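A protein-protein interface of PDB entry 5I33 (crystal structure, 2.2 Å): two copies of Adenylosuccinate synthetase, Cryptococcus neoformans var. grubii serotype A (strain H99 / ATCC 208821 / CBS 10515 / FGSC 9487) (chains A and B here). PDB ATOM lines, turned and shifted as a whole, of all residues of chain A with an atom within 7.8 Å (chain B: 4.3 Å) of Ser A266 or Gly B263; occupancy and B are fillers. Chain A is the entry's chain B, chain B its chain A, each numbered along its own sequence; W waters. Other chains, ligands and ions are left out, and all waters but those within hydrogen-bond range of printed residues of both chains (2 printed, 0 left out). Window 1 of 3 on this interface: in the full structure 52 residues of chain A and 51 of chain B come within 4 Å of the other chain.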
ATOM      1  N   CYS A  49     -13.319 -11.103   8.303  1.00  0.00           N
ATOM      2  CA  CYS A  49     -13.727 -11.410   6.936  1.00  0.00           C
ATOM      3  C   CYS A  49     -14.833 -12.465   6.894  1.00  0.00           C
ATOM      4  O   CYS A  49     -15.653 -12.459   5.977  1.00  0.00           O
ATOM      5  CB  CYS A  49     -12.516 -11.885   6.126  1.00  0.00           C
ATOM      6  SG  CYS A  49     -11.678 -13.391   6.942  1.00  0.00           S
ATOM      7  N   ALA A  50     -14.861 -13.357   7.894  1.00  0.00           N
ATOM      8  CA  ALA A  50     -15.793 -14.494   7.909  1.00  0.00           C
ATOM      9  C   ALA A  50     -16.088 -14.954   9.327  1.00  0.00           C
ATOM     10  O   ALA A  50     -15.440 -14.519  10.269  1.00  0.00           O
ATOM     11  CB  ALA A  50     -15.236 -15.653   7.098  1.00  0.00           C
ATOM     12  N   GLY A  90     -16.303  -7.327   7.407  1.00  0.00           N
ATOM     13  CA  GLY A  90     -16.480  -7.684   6.001  1.00  0.00           C
ATOM     14  C   GLY A  90     -17.796  -8.352   5.635  1.00  0.00           C
ATOM     15  O   GLY A  90     -18.574  -8.711   6.521  1.00  0.00           O
ATOM     16  N   SER A  91     -18.045  -8.534   4.334  1.00  0.00           N
ATOM     17  CA  SER A  91     -19.332  -9.074   3.874  1.00  0.00           C
ATOM     18  C   SER A  91     -19.518 -10.564   4.188  1.00  0.00           C
ATOM     19  O   SER A  91     -20.646 -11.049   4.297  1.00  0.00           O
ATOM     20  CB  SER A  91     -19.513  -8.834   2.366  1.00  0.00           C
ATOM     21  OG  SER A  91     -19.391  -7.446   2.060  1.00  0.00           O
ATOM     22  N   GLY A  92     -18.417 -11.276   4.380  1.00  0.00           N
ATOM     23  CA  GLY A  92     -18.457 -12.711   4.661  1.00  0.00           C
ATOM     24  C   GLY A  92     -18.879 -13.067   6.082  1.00  0.00           C
ATOM     25  O   GLY A  92     -19.150 -14.227   6.396  1.00  0.00           O
ATOM     26  N   VAL A  93     -18.925 -12.065   6.950  1.00  0.00           N
ATOM     27  CA  VAL A  93     -19.292 -12.265   8.350  1.00  0.00           C
ATOM     28  C   VAL A  93     -20.823 -12.429   8.538  1.00  0.00           C
ATOM     29  O   VAL A  93     -21.614 -11.967   7.706  1.00  0.00           O
ATOM     30  CB  VAL A  93     -18.768 -11.081   9.185  1.00  0.00           C
ATOM     31  CG1 VAL A  93     -19.075 -11.268  10.668  1.00  0.00           C
ATOM     32  CG2 VAL A  93     -17.275 -10.962   9.009  1.00  0.00           C
ATOM     33  N   LYS A 161     -28.327 -17.959   4.481  1.00  0.00           N
ATOM     34  CA  LYS A 161     -27.535 -17.294   3.455  1.00  0.00           C
ATOM     35  C   LYS A 161     -27.467 -18.140   2.189  1.00  0.00           C
ATOM     36  O   LYS A 161     -27.746 -17.654   1.086  1.00  0.00           O
ATOM     37  CB  LYS A 161     -26.135 -16.996   3.975  1.00  0.00           C
ATOM     38  CG  LYS A 161     -25.204 -16.341   2.973  1.00  0.00           C
ATOM     39  CD  LYS A 161     -23.867 -16.004   3.600  1.00  0.00           C
ATOM     40  CE  LYS A 161     -22.969 -15.305   2.596  1.00  0.00           C
ATOM     41  NZ  LYS A 161     -21.666 -14.897   3.194  1.00  0.00           N
ATOM     42  N   ASP A 247     -14.758 -26.465   4.719  1.00  0.00           N
ATOM     43  CA  ASP A 247     -14.343 -27.399   3.673  1.00  0.00           C
ATOM     44  C   ASP A 247     -13.276 -28.391   4.153  1.00  0.00           C
ATOM     45  O   ASP A 247     -13.372 -29.593   3.900  1.00  0.00           O
ATOM     46  CB  ASP A 247     -13.787 -26.669   2.450  1.00  0.00           C
ATOM     47  CG  ASP A 247     -14.866 -25.996   1.612  1.00  0.00           C
ATOM     48  OD1 ASP A 247     -15.697 -26.713   1.000  1.00  0.00           O
ATOM     49  OD2 ASP A 247     -14.841 -24.752   1.545  1.00  0.00           O
ATOM     50  N   TYR A 248     -12.251 -27.872   4.822  1.00  0.00           N
ATOM     51  CA  TYR A 248     -11.002 -28.599   4.937  1.00  0.00           C
ATOM     52  C   TYR A 248     -10.702 -29.132   6.342  1.00  0.00           C
ATOM     53  O   TYR A 248      -9.690 -29.789   6.546  1.00  0.00           O
ATOM     54  CB  TYR A 248      -9.868 -27.705   4.427  1.00  0.00           C
ATOM     55  CG  TYR A 248     -10.064 -27.440   2.958  1.00  0.00           C
ATOM     56  CD1 TYR A 248     -10.022 -28.485   2.040  1.00  0.00           C
ATOM     57  CD2 TYR A 248     -10.345 -26.157   2.490  1.00  0.00           C
ATOM     58  CE1 TYR A 248     -10.242 -28.260   0.683  1.00  0.00           C
ATOM     59  CE2 TYR A 248     -10.554 -25.915   1.147  1.00  0.00           C
ATOM     60  CZ  TYR A 248     -10.509 -26.959   0.238  1.00  0.00           C
ATOM     61  OH  TYR A 248     -10.733 -26.715  -1.115  1.00  0.00           O
ATOM     62  N   SER A 258     -15.817 -20.604   6.057  1.00  0.00           N
ATOM     63  CA  SER A 258     -14.370 -20.669   5.887  1.00  0.00           C
ATOM     64  C   SER A 258     -13.603 -20.011   7.041  1.00  0.00           C
ATOM     65  O   SER A 258     -13.940 -18.911   7.483  1.00  0.00           O
ATOM     66  CB  SER A 258     -13.933 -20.026   4.581  1.00  0.00           C
ATOM     67  OG  SER A 258     -12.512 -20.042   4.504  1.00  0.00           O
ATOM     68  N   SER A 260     -10.194 -20.310   6.631  1.00  0.00           N
ATOM     69  CA  SER A 260      -8.919 -20.289   5.925  1.00  0.00           C
ATOM     70  C   SER A 260      -8.754 -19.107   4.963  1.00  0.00           C
ATOM     71  O   SER A 260      -9.586 -18.203   4.910  1.00  0.00           O
ATOM     72  CB  SER A 260      -8.748 -21.587   5.163  1.00  0.00           C
ATOM     73  OG  SER A 260      -9.971 -21.984   4.584  1.00  0.00           O
ATOM     74  N   ILE A 261      -7.662 -19.125   4.211  1.00  0.00           N
ATOM     75  CA  ILE A 261      -7.229 -17.950   3.469  1.00  0.00           C
ATOM     76  C   ILE A 261      -8.249 -17.553   2.365  1.00  0.00           C
ATOM     77  O   ILE A 261      -8.390 -16.373   2.050  1.00  0.00           O
ATOM     78  CB  ILE A 261      -5.832 -18.185   2.866  1.00  0.00           C
ATOM     79  CG1 ILE A 261      -5.235 -16.894   2.289  1.00  0.00           C
ATOM     80  CG2 ILE A 261      -5.889 -19.334   1.831  1.00  0.00           C
ATOM     81  CD1 ILE A 261      -5.160 -15.725   3.255  1.00  0.00           C
ATOM     82  N   GLY A 262      -8.961 -18.532   1.801  1.00  0.00           N
ATOM     83  CA  GLY A 262      -9.983 -18.257   0.798  1.00  0.00           C
ATOM     84  C   GLY A 262     -11.142 -17.428   1.341  1.00  0.00           C
ATOM     85  O   GLY A 262     -11.752 -16.606   0.619  1.00  0.00           O
ATOM     86  N   GLY A 263     -11.449 -17.657   2.619  1.00  0.00           N
ATOM     87  CA  GLY A 263     -12.482 -16.920   3.320  1.00  0.00           C
ATOM     88  C   GLY A 263     -12.128 -15.453   3.450  1.00  0.00           C
ATOM     89  O   GLY A 263     -13.007 -14.576   3.535  1.00  0.00           O
ATOM     90  N   VAL A 264     -10.830 -15.175   3.459  1.00  0.00           N
ATOM     91  CA  VAL A 264     -10.369 -13.793   3.501  1.00  0.00           C
ATOM     92  C   VAL A 264     -10.599 -13.127   2.133  1.00  0.00           C
ATOM     93  O   VAL A 264     -11.112 -12.010   2.063  1.00  0.00           O
ATOM     94  CB  VAL A 264      -8.876 -13.702   3.897  1.00  0.00           C
ATOM     95  CG1 VAL A 264      -8.475 -12.257   4.075  1.00  0.00           C
ATOM     96  CG2 VAL A 264      -8.634 -14.460   5.189  1.00  0.00           C
ATOM     97  N   VAL A 265     -10.217 -13.809   1.055  1.00  0.00           N
ATOM     98  CA  VAL A 265     -10.419 -13.276  -0.284  1.00  0.00           C
ATOM     99  C   VAL A 265     -11.914 -13.050  -0.580  1.00  0.00           C
ATOM    100  O   VAL A 265     -12.306 -11.983  -1.048  1.00  0.00           O
ATOM    101  CB  VAL A 265      -9.833 -14.202  -1.344  1.00  0.00           C
ATOM    102  CG1 VAL A 265     -10.033 -13.590  -2.732  1.00  0.00           C
ATOM    103  CG2 VAL A 265      -8.341 -14.471  -1.052  1.00  0.00           C
ATOM    104  N   SER A 266     -12.732 -14.058  -0.285  1.00  0.00           N
ATOM    105  CA  SER A 266     -14.185 -13.993  -0.439  1.00  0.00           C
ATOM    106  C   SER A 266     -14.810 -12.971   0.480  1.00  0.00           C
ATOM    107  O   SER A 266     -15.623 -12.158   0.037  1.00  0.00           O
ATOM    108  CB  SER A 266     -14.850 -15.352  -0.165  1.00  0.00           C
ATOM    109  OG  SER A 266     -14.556 -16.296  -1.176  1.00  0.00           O
ATOM    110  N   GLY A 267     -14.458 -13.046   1.761  1.00  0.00           N
ATOM    111  CA  GLY A 267     -15.070 -12.224   2.796  1.00  0.00           C
ATOM    112  C   GLY A 267     -14.765 -10.726   2.757  1.00  0.00           C
ATOM    113  O   GLY A 267     -15.527  -9.924   3.317  1.00  0.00           O
ATOM    114  N   LEU A 268     -13.647 -10.343   2.138  1.00  0.00           N
ATOM    115  CA  LEU A 268     -13.340  -8.928   1.951  1.00  0.00           C
ATOM    116  C   LEU A 268     -13.588  -8.472   0.510  1.00  0.00           C
ATOM    117  O   LEU A 268     -13.569  -7.271   0.235  1.00  0.00           O
ATOM    118  CB  LEU A 268     -11.899  -8.627   2.329  1.00  0.00           C
ATOM    119  CG  LEU A 268     -11.523  -8.936   3.781  1.00  0.00           C
ATOM    120  CD1 LEU A 268     -10.048  -8.625   4.014  1.00  0.00           C
ATOM    121  CD2 LEU A 268     -12.406  -8.148   4.739  1.00  0.00           C
ATOM    122  N   GLY A 269     -13.826  -9.426  -0.391  1.00  0.00           N
ATOM    123  CA  GLY A 269     -14.074  -9.130  -1.799  1.00  0.00           C
ATOM    124  C   GLY A 269     -12.867  -8.484  -2.441  1.00  0.00           C
ATOM    125  O   GLY A 269     -12.979  -7.461  -3.108  1.00  0.00           O
ATOM    126  N   ILE A 270     -11.686  -9.043  -2.189  1.00  0.00           N
ATOM    127  CA  ILE A 270     -10.470  -8.485  -2.772  1.00  0.00           C
ATOM    128  C   ILE A 270      -9.793  -9.474  -3.714  1.00  0.00           C
ATOM    129  O   ILE A 270     -10.169 -10.642  -3.773  1.00  0.00           O
ATOM    130  CB  ILE A 270      -9.466  -8.054  -1.679  1.00  0.00           C
ATOM    131  CG1 ILE A 270      -9.074  -9.228  -0.771  1.00  0.00           C
ATOM    132  CG2 ILE A 270     -10.054  -6.926  -0.856  1.00  0.00           C
ATOM    133  CD1 ILE A 270      -7.984  -8.873   0.225  1.00  0.00           C
ATOM    134  N   SER A 271      -8.806  -8.991  -4.459  1.00  0.00           N
ATOM    135  CA  SER A 271      -7.978  -9.842  -5.309  1.00  0.00           C
ATOM    136  C   SER A 271      -6.998 -10.693  -4.485  1.00  0.00           C
ATOM    137  O   SER A 271      -6.440 -10.199  -3.506  1.00  0.00           O
ATOM    138  CB  SER A 271      -7.181  -8.986  -6.289  1.00  0.00           C
ATOM    139  OG  SER A 271      -6.228  -9.770  -6.986  1.00  0.00           O
ATOM    140  N   CYS B  49     -14.146 -25.378  -9.288  1.00  0.00           N
ATOM    141  CA  CYS B  49     -13.778 -25.093  -7.902  1.00  0.00           C
ATOM    142  C   CYS B  49     -14.995 -24.943  -6.985  1.00  0.00           C
ATOM    143  O   CYS B  49     -14.908 -25.187  -5.769  1.00  0.00           O
ATOM    144  CB  CYS B  49     -12.934 -23.818  -7.842  1.00  0.00           C
ATOM    145  SG  CYS B  49     -13.819 -22.375  -8.562  1.00  0.00           S
ATOM    146  N   ALA B  50     -16.110 -24.506  -7.566  1.00  0.00           N
ATOM    147  CA  ALA B  50     -17.321 -24.189  -6.815  1.00  0.00           C
ATOM    148  C   ALA B  50     -18.586 -24.246  -7.690  1.00  0.00           C
ATOM    149  O   ALA B  50     -18.506 -24.283  -8.918  1.00  0.00           O
ATOM    150  CB  ALA B  50     -17.185 -22.800  -6.175  1.00  0.00           C
ATOM    151  N   TYR B 248     -21.677 -10.956  -3.447  1.00  0.00           N
ATOM    152  CA  TYR B 248     -21.453  -9.677  -4.066  1.00  0.00           C
ATOM    153  C   TYR B 248     -22.396  -9.384  -5.220  1.00  0.00           C
ATOM    154  O   TYR B 248     -22.356  -8.301  -5.765  1.00  0.00           O
ATOM    155  CB  TYR B 248     -20.001  -9.593  -4.529  1.00  0.00           C
ATOM    156  CG  TYR B 248     -19.085  -9.609  -3.353  1.00  0.00           C
ATOM    157  CD1 TYR B 248     -19.106  -8.571  -2.433  1.00  0.00           C
ATOM    158  CD2 TYR B 248     -18.254 -10.701  -3.105  1.00  0.00           C
ATOM    159  CE1 TYR B 248     -18.288  -8.587  -1.311  1.00  0.00           C
ATOM    160  CE2 TYR B 248     -17.433 -10.739  -1.972  1.00  0.00           C
ATOM    161  CZ  TYR B 248     -17.456  -9.682  -1.080  1.00  0.00           C
ATOM    162  OH  TYR B 248     -16.644  -9.709   0.033  1.00  0.00           O
ATOM    163  N   SER B 258     -20.044 -18.877  -4.021  1.00  0.00           N
ATOM    164  CA  SER B 258     -19.111 -17.958  -4.653  1.00  0.00           C
ATOM    165  C   SER B 258     -18.929 -18.299  -6.120  1.00  0.00           C
ATOM    166  O   SER B 258     -18.800 -19.472  -6.487  1.00  0.00           O
ATOM    167  CB  SER B 258     -17.758 -17.965  -3.949  1.00  0.00           C
ATOM    168  OG  SER B 258     -16.846 -17.111  -4.625  1.00  0.00           O
ATOM    169  N   SER B 260     -16.902 -15.969  -7.673  1.00  0.00           N
ATOM    170  CA  SER B 260     -15.751 -15.102  -7.818  1.00  0.00           C
ATOM    171  C   SER B 260     -14.444 -15.729  -7.347  1.00  0.00           C
ATOM    172  O   SER B 260     -14.388 -16.904  -6.944  1.00  0.00           O
ATOM    173  CB  SER B 260     -15.991 -13.821  -7.046  1.00  0.00           C
ATOM    174  OG  SER B 260     -16.646 -14.144  -5.843  1.00  0.00           O
ATOM    175  N   ILE B 261     -13.403 -14.905  -7.381  1.00  0.00           N
ATOM    176  CA  ILE B 261     -12.045 -15.395  -7.314  1.00  0.00           C
ATOM    177  C   ILE B 261     -11.778 -16.078  -5.949  1.00  0.00           C
ATOM    178  O   ILE B 261     -11.070 -17.068  -5.895  1.00  0.00           O
ATOM    179  CB  ILE B 261     -11.038 -14.242  -7.613  1.00  0.00           C
ATOM    180  CG1 ILE B 261      -9.605 -14.786  -7.722  1.00  0.00           C
ATOM    181  CG2 ILE B 261     -11.166 -13.122  -6.595  1.00  0.00           C
ATOM    182  CD1 ILE B 261      -9.465 -15.882  -8.774  1.00  0.00           C
ATOM    183  N   GLY B 262     -12.428 -15.606  -4.890  1.00  0.00           N
ATOM    184  CA  GLY B 262     -12.304 -16.219  -3.582  1.00  0.00           C
ATOM    185  C   GLY B 262     -12.785 -17.658  -3.538  1.00  0.00           C
ATOM    186  O   GLY B 262     -12.225 -18.504  -2.817  1.00  0.00           O
ATOM    187  N   GLY B 263     -13.816 -17.944  -4.322  1.00  0.00           N
ATOM    188  CA  GLY B 263     -14.350 -19.282  -4.449  1.00  0.00           C
ATOM    189  C   GLY B 263     -13.337 -20.235  -5.062  1.00  0.00           C
ATOM    190  O   GLY B 263     -13.389 -21.457  -4.825  1.00  0.00           O
ATOM    191  N   VAL B 264     -12.416 -19.692  -5.854  1.00  0.00           N
ATOM    192  CA  VAL B 264     -11.359 -20.505  -6.458  1.00  0.00           C
ATOM    193  C   VAL B 264     -10.317 -20.921  -5.420  1.00  0.00           C
ATOM    194  O   VAL B 264      -9.940 -22.082  -5.348  1.00  0.00           O
ATOM    195  CB  VAL B 264     -10.625 -19.766  -7.600  1.00  0.00           C
ATOM    196  CG1 VAL B 264      -9.562 -20.672  -8.206  1.00  0.00           C
ATOM    197  CG2 VAL B 264     -11.618 -19.264  -8.677  1.00  0.00           C
ATOM    198  N   VAL B 265      -9.857 -19.949  -4.636  1.00  0.00           N
ATOM    199  CA  VAL B 265      -8.884 -20.187  -3.587  1.00  0.00           C
ATOM    200  C   VAL B 265      -9.443 -21.192  -2.580  1.00  0.00           C
ATOM    201  O   VAL B 265      -8.790 -22.169  -2.253  1.00  0.00           O
ATOM    202  CB  VAL B 265      -8.502 -18.868  -2.867  1.00  0.00           C
ATOM    203  CG1 VAL B 265      -7.516 -19.117  -1.726  1.00  0.00           C
ATOM    204  CG2 VAL B 265      -7.934 -17.876  -3.863  1.00  0.00           C
ATOM    205  N   SER B 266     -10.673 -20.950  -2.141  1.00  0.00           N
ATOM    206  CA  SER B 266     -11.388 -21.834  -1.223  1.00  0.00           C
ATOM    207  C   SER B 266     -11.693 -23.200  -1.812  1.00  0.00           C
ATOM    208  O   SER B 266     -11.404 -24.216  -1.195  1.00  0.00           O
ATOM    209  CB  SER B 266     -12.713 -21.194  -0.790  1.00  0.00           C
ATOM    210  OG  SER B 266     -12.484 -20.072   0.031  1.00  0.00           O
ATOM    211  N   GLY B 267     -12.288 -23.206  -3.000  1.00  0.00           N
ATOM    212  CA  GLY B 267     -12.790 -24.424  -3.599  1.00  0.00           C
ATOM    213  C   GLY B 267     -11.741 -25.420  -4.043  1.00  0.00           C
ATOM    214  O   GLY B 267     -12.045 -26.602  -4.186  1.00  0.00           O
HETATM  215  O   HOH W   1     -12.021 -21.133   2.351  1.00  0.00           O
HETATM  216  O   HOH W   2     -14.871 -18.545  -0.238  1.00  0.00           O
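Among the printed residues, pairs that only touch across the chains: Gly A262 with Ser B266 (3.2 Å), Ser A266 with Gly B262 (3.3 Å), Leu A268 with Tyr B248 (3.3 Å), Val A265 with Gly B262 (3.6 Å), Ser A266 with Gly B263 (3.6 Å), Gly A262 with Val B265 (3.6 Å), Gly A263 with Ser B266 (3.7 Å), Ser A91 with Tyr B248 (3.7 Å), Ile A270 with Ile B261 (3.9 Å), Ile A261 with Val B265 (3.9 Å) and Gly A262 with Gly B262 (3.95 Å).
Water W2 lies within hydrogen-bond range of OG of Ser A266 (2.5 Å) and OG of Ser B266 (2.8 Å). Water W1 lies within hydrogen-bond range of OG of Ser A258 (2.5 Å), OG of Ser B266 (2.6 Å) and OG of Ser A260 (3.1 Å).
Printed residues of chain B within 4 Å of Ser A91: Tyr B248. Of the printed residues of chain B, Gly A262 touches Gly B262, Val B265 and Ser B266. Ser A266 touches just these residues of chain B: Tyr B248 (2.7 Å), Gly B262 (3.3 Å) and Gly B263 (3.6 Å). Gly B263 touches just one residue of chain A: Ser A266 (3.6 Å). Printed residues of chain A within 4 Å of Val B265: Ile A261 and Gly A262.
The backbone NH (N) of Gly A92 is in hydrogen-bond range of the backbone carbonyl oxygen (O) of Gly A267 (3.4 Å). The side-chain hydroxyl (OG) of Ser B258 is in hydrogen-bond range of the backbone NH (N) of Gly B263. N of Gly A263 lies within hydrogen-bond range of OG of Ser A258 (3.2 Å). O of Val A265 sits at hydrogen-bond distance from N of Ile A270, 3.2 Å away. The backbone carbonyl oxygen (O) of Gly B262 sits at hydrogen-bond distance from the side-chain hydroxyl (OG) of Ser B266 (3.3 Å). O of Gly A267 is in hydrogen-bond range of N of Ser A91 (3.1 Å).
Hydrophobic or aromatic side chains of chain A within 4 Å of the printed part of chain B: Tyr A248, Ile A261 and Val A265. Of the 12 printed residues of chain B, 7 touch a printed residue of chain A.
The backbone carbonyl oxygen (O) of Gly A267 sits close to the side-chain hydroxyl (OH) of Tyr B248 (3.5 Å). OH of Tyr B248 sits at hydrogen-bond distance from N of Gly A269 (2.9 Å). OH of Tyr B248 is in hydrogen-bond range of O of Ser A266, 2.7 Å away. The backbone carbonyl oxygen (O) of Ser B266 is in hydrogen-bond range of the side-chain hydroxyl (OH) of Tyr A248. The backbone carbonyl oxygen of Gly B267 is in hydrogen-bond range of the side-chain hydroxyl of Tyr A248, 3.3 Å away.
Tyr A248 touches Ser B266, and with the chains exchanged Ser A266 touches Tyr B248. Tyr A248 touches Gly B267, and with the chains exchanged Gly A267 touches Tyr B248. Gly A262 touches its own counterpart, Gly B262. Gly A262 touches Val B265, and with the chains exchanged Val A265 touches Gly B262. Positions printed for both chains: 49, 50, 248, 258, 260, 261, 262, 263, 264, 265, 266 and 267.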
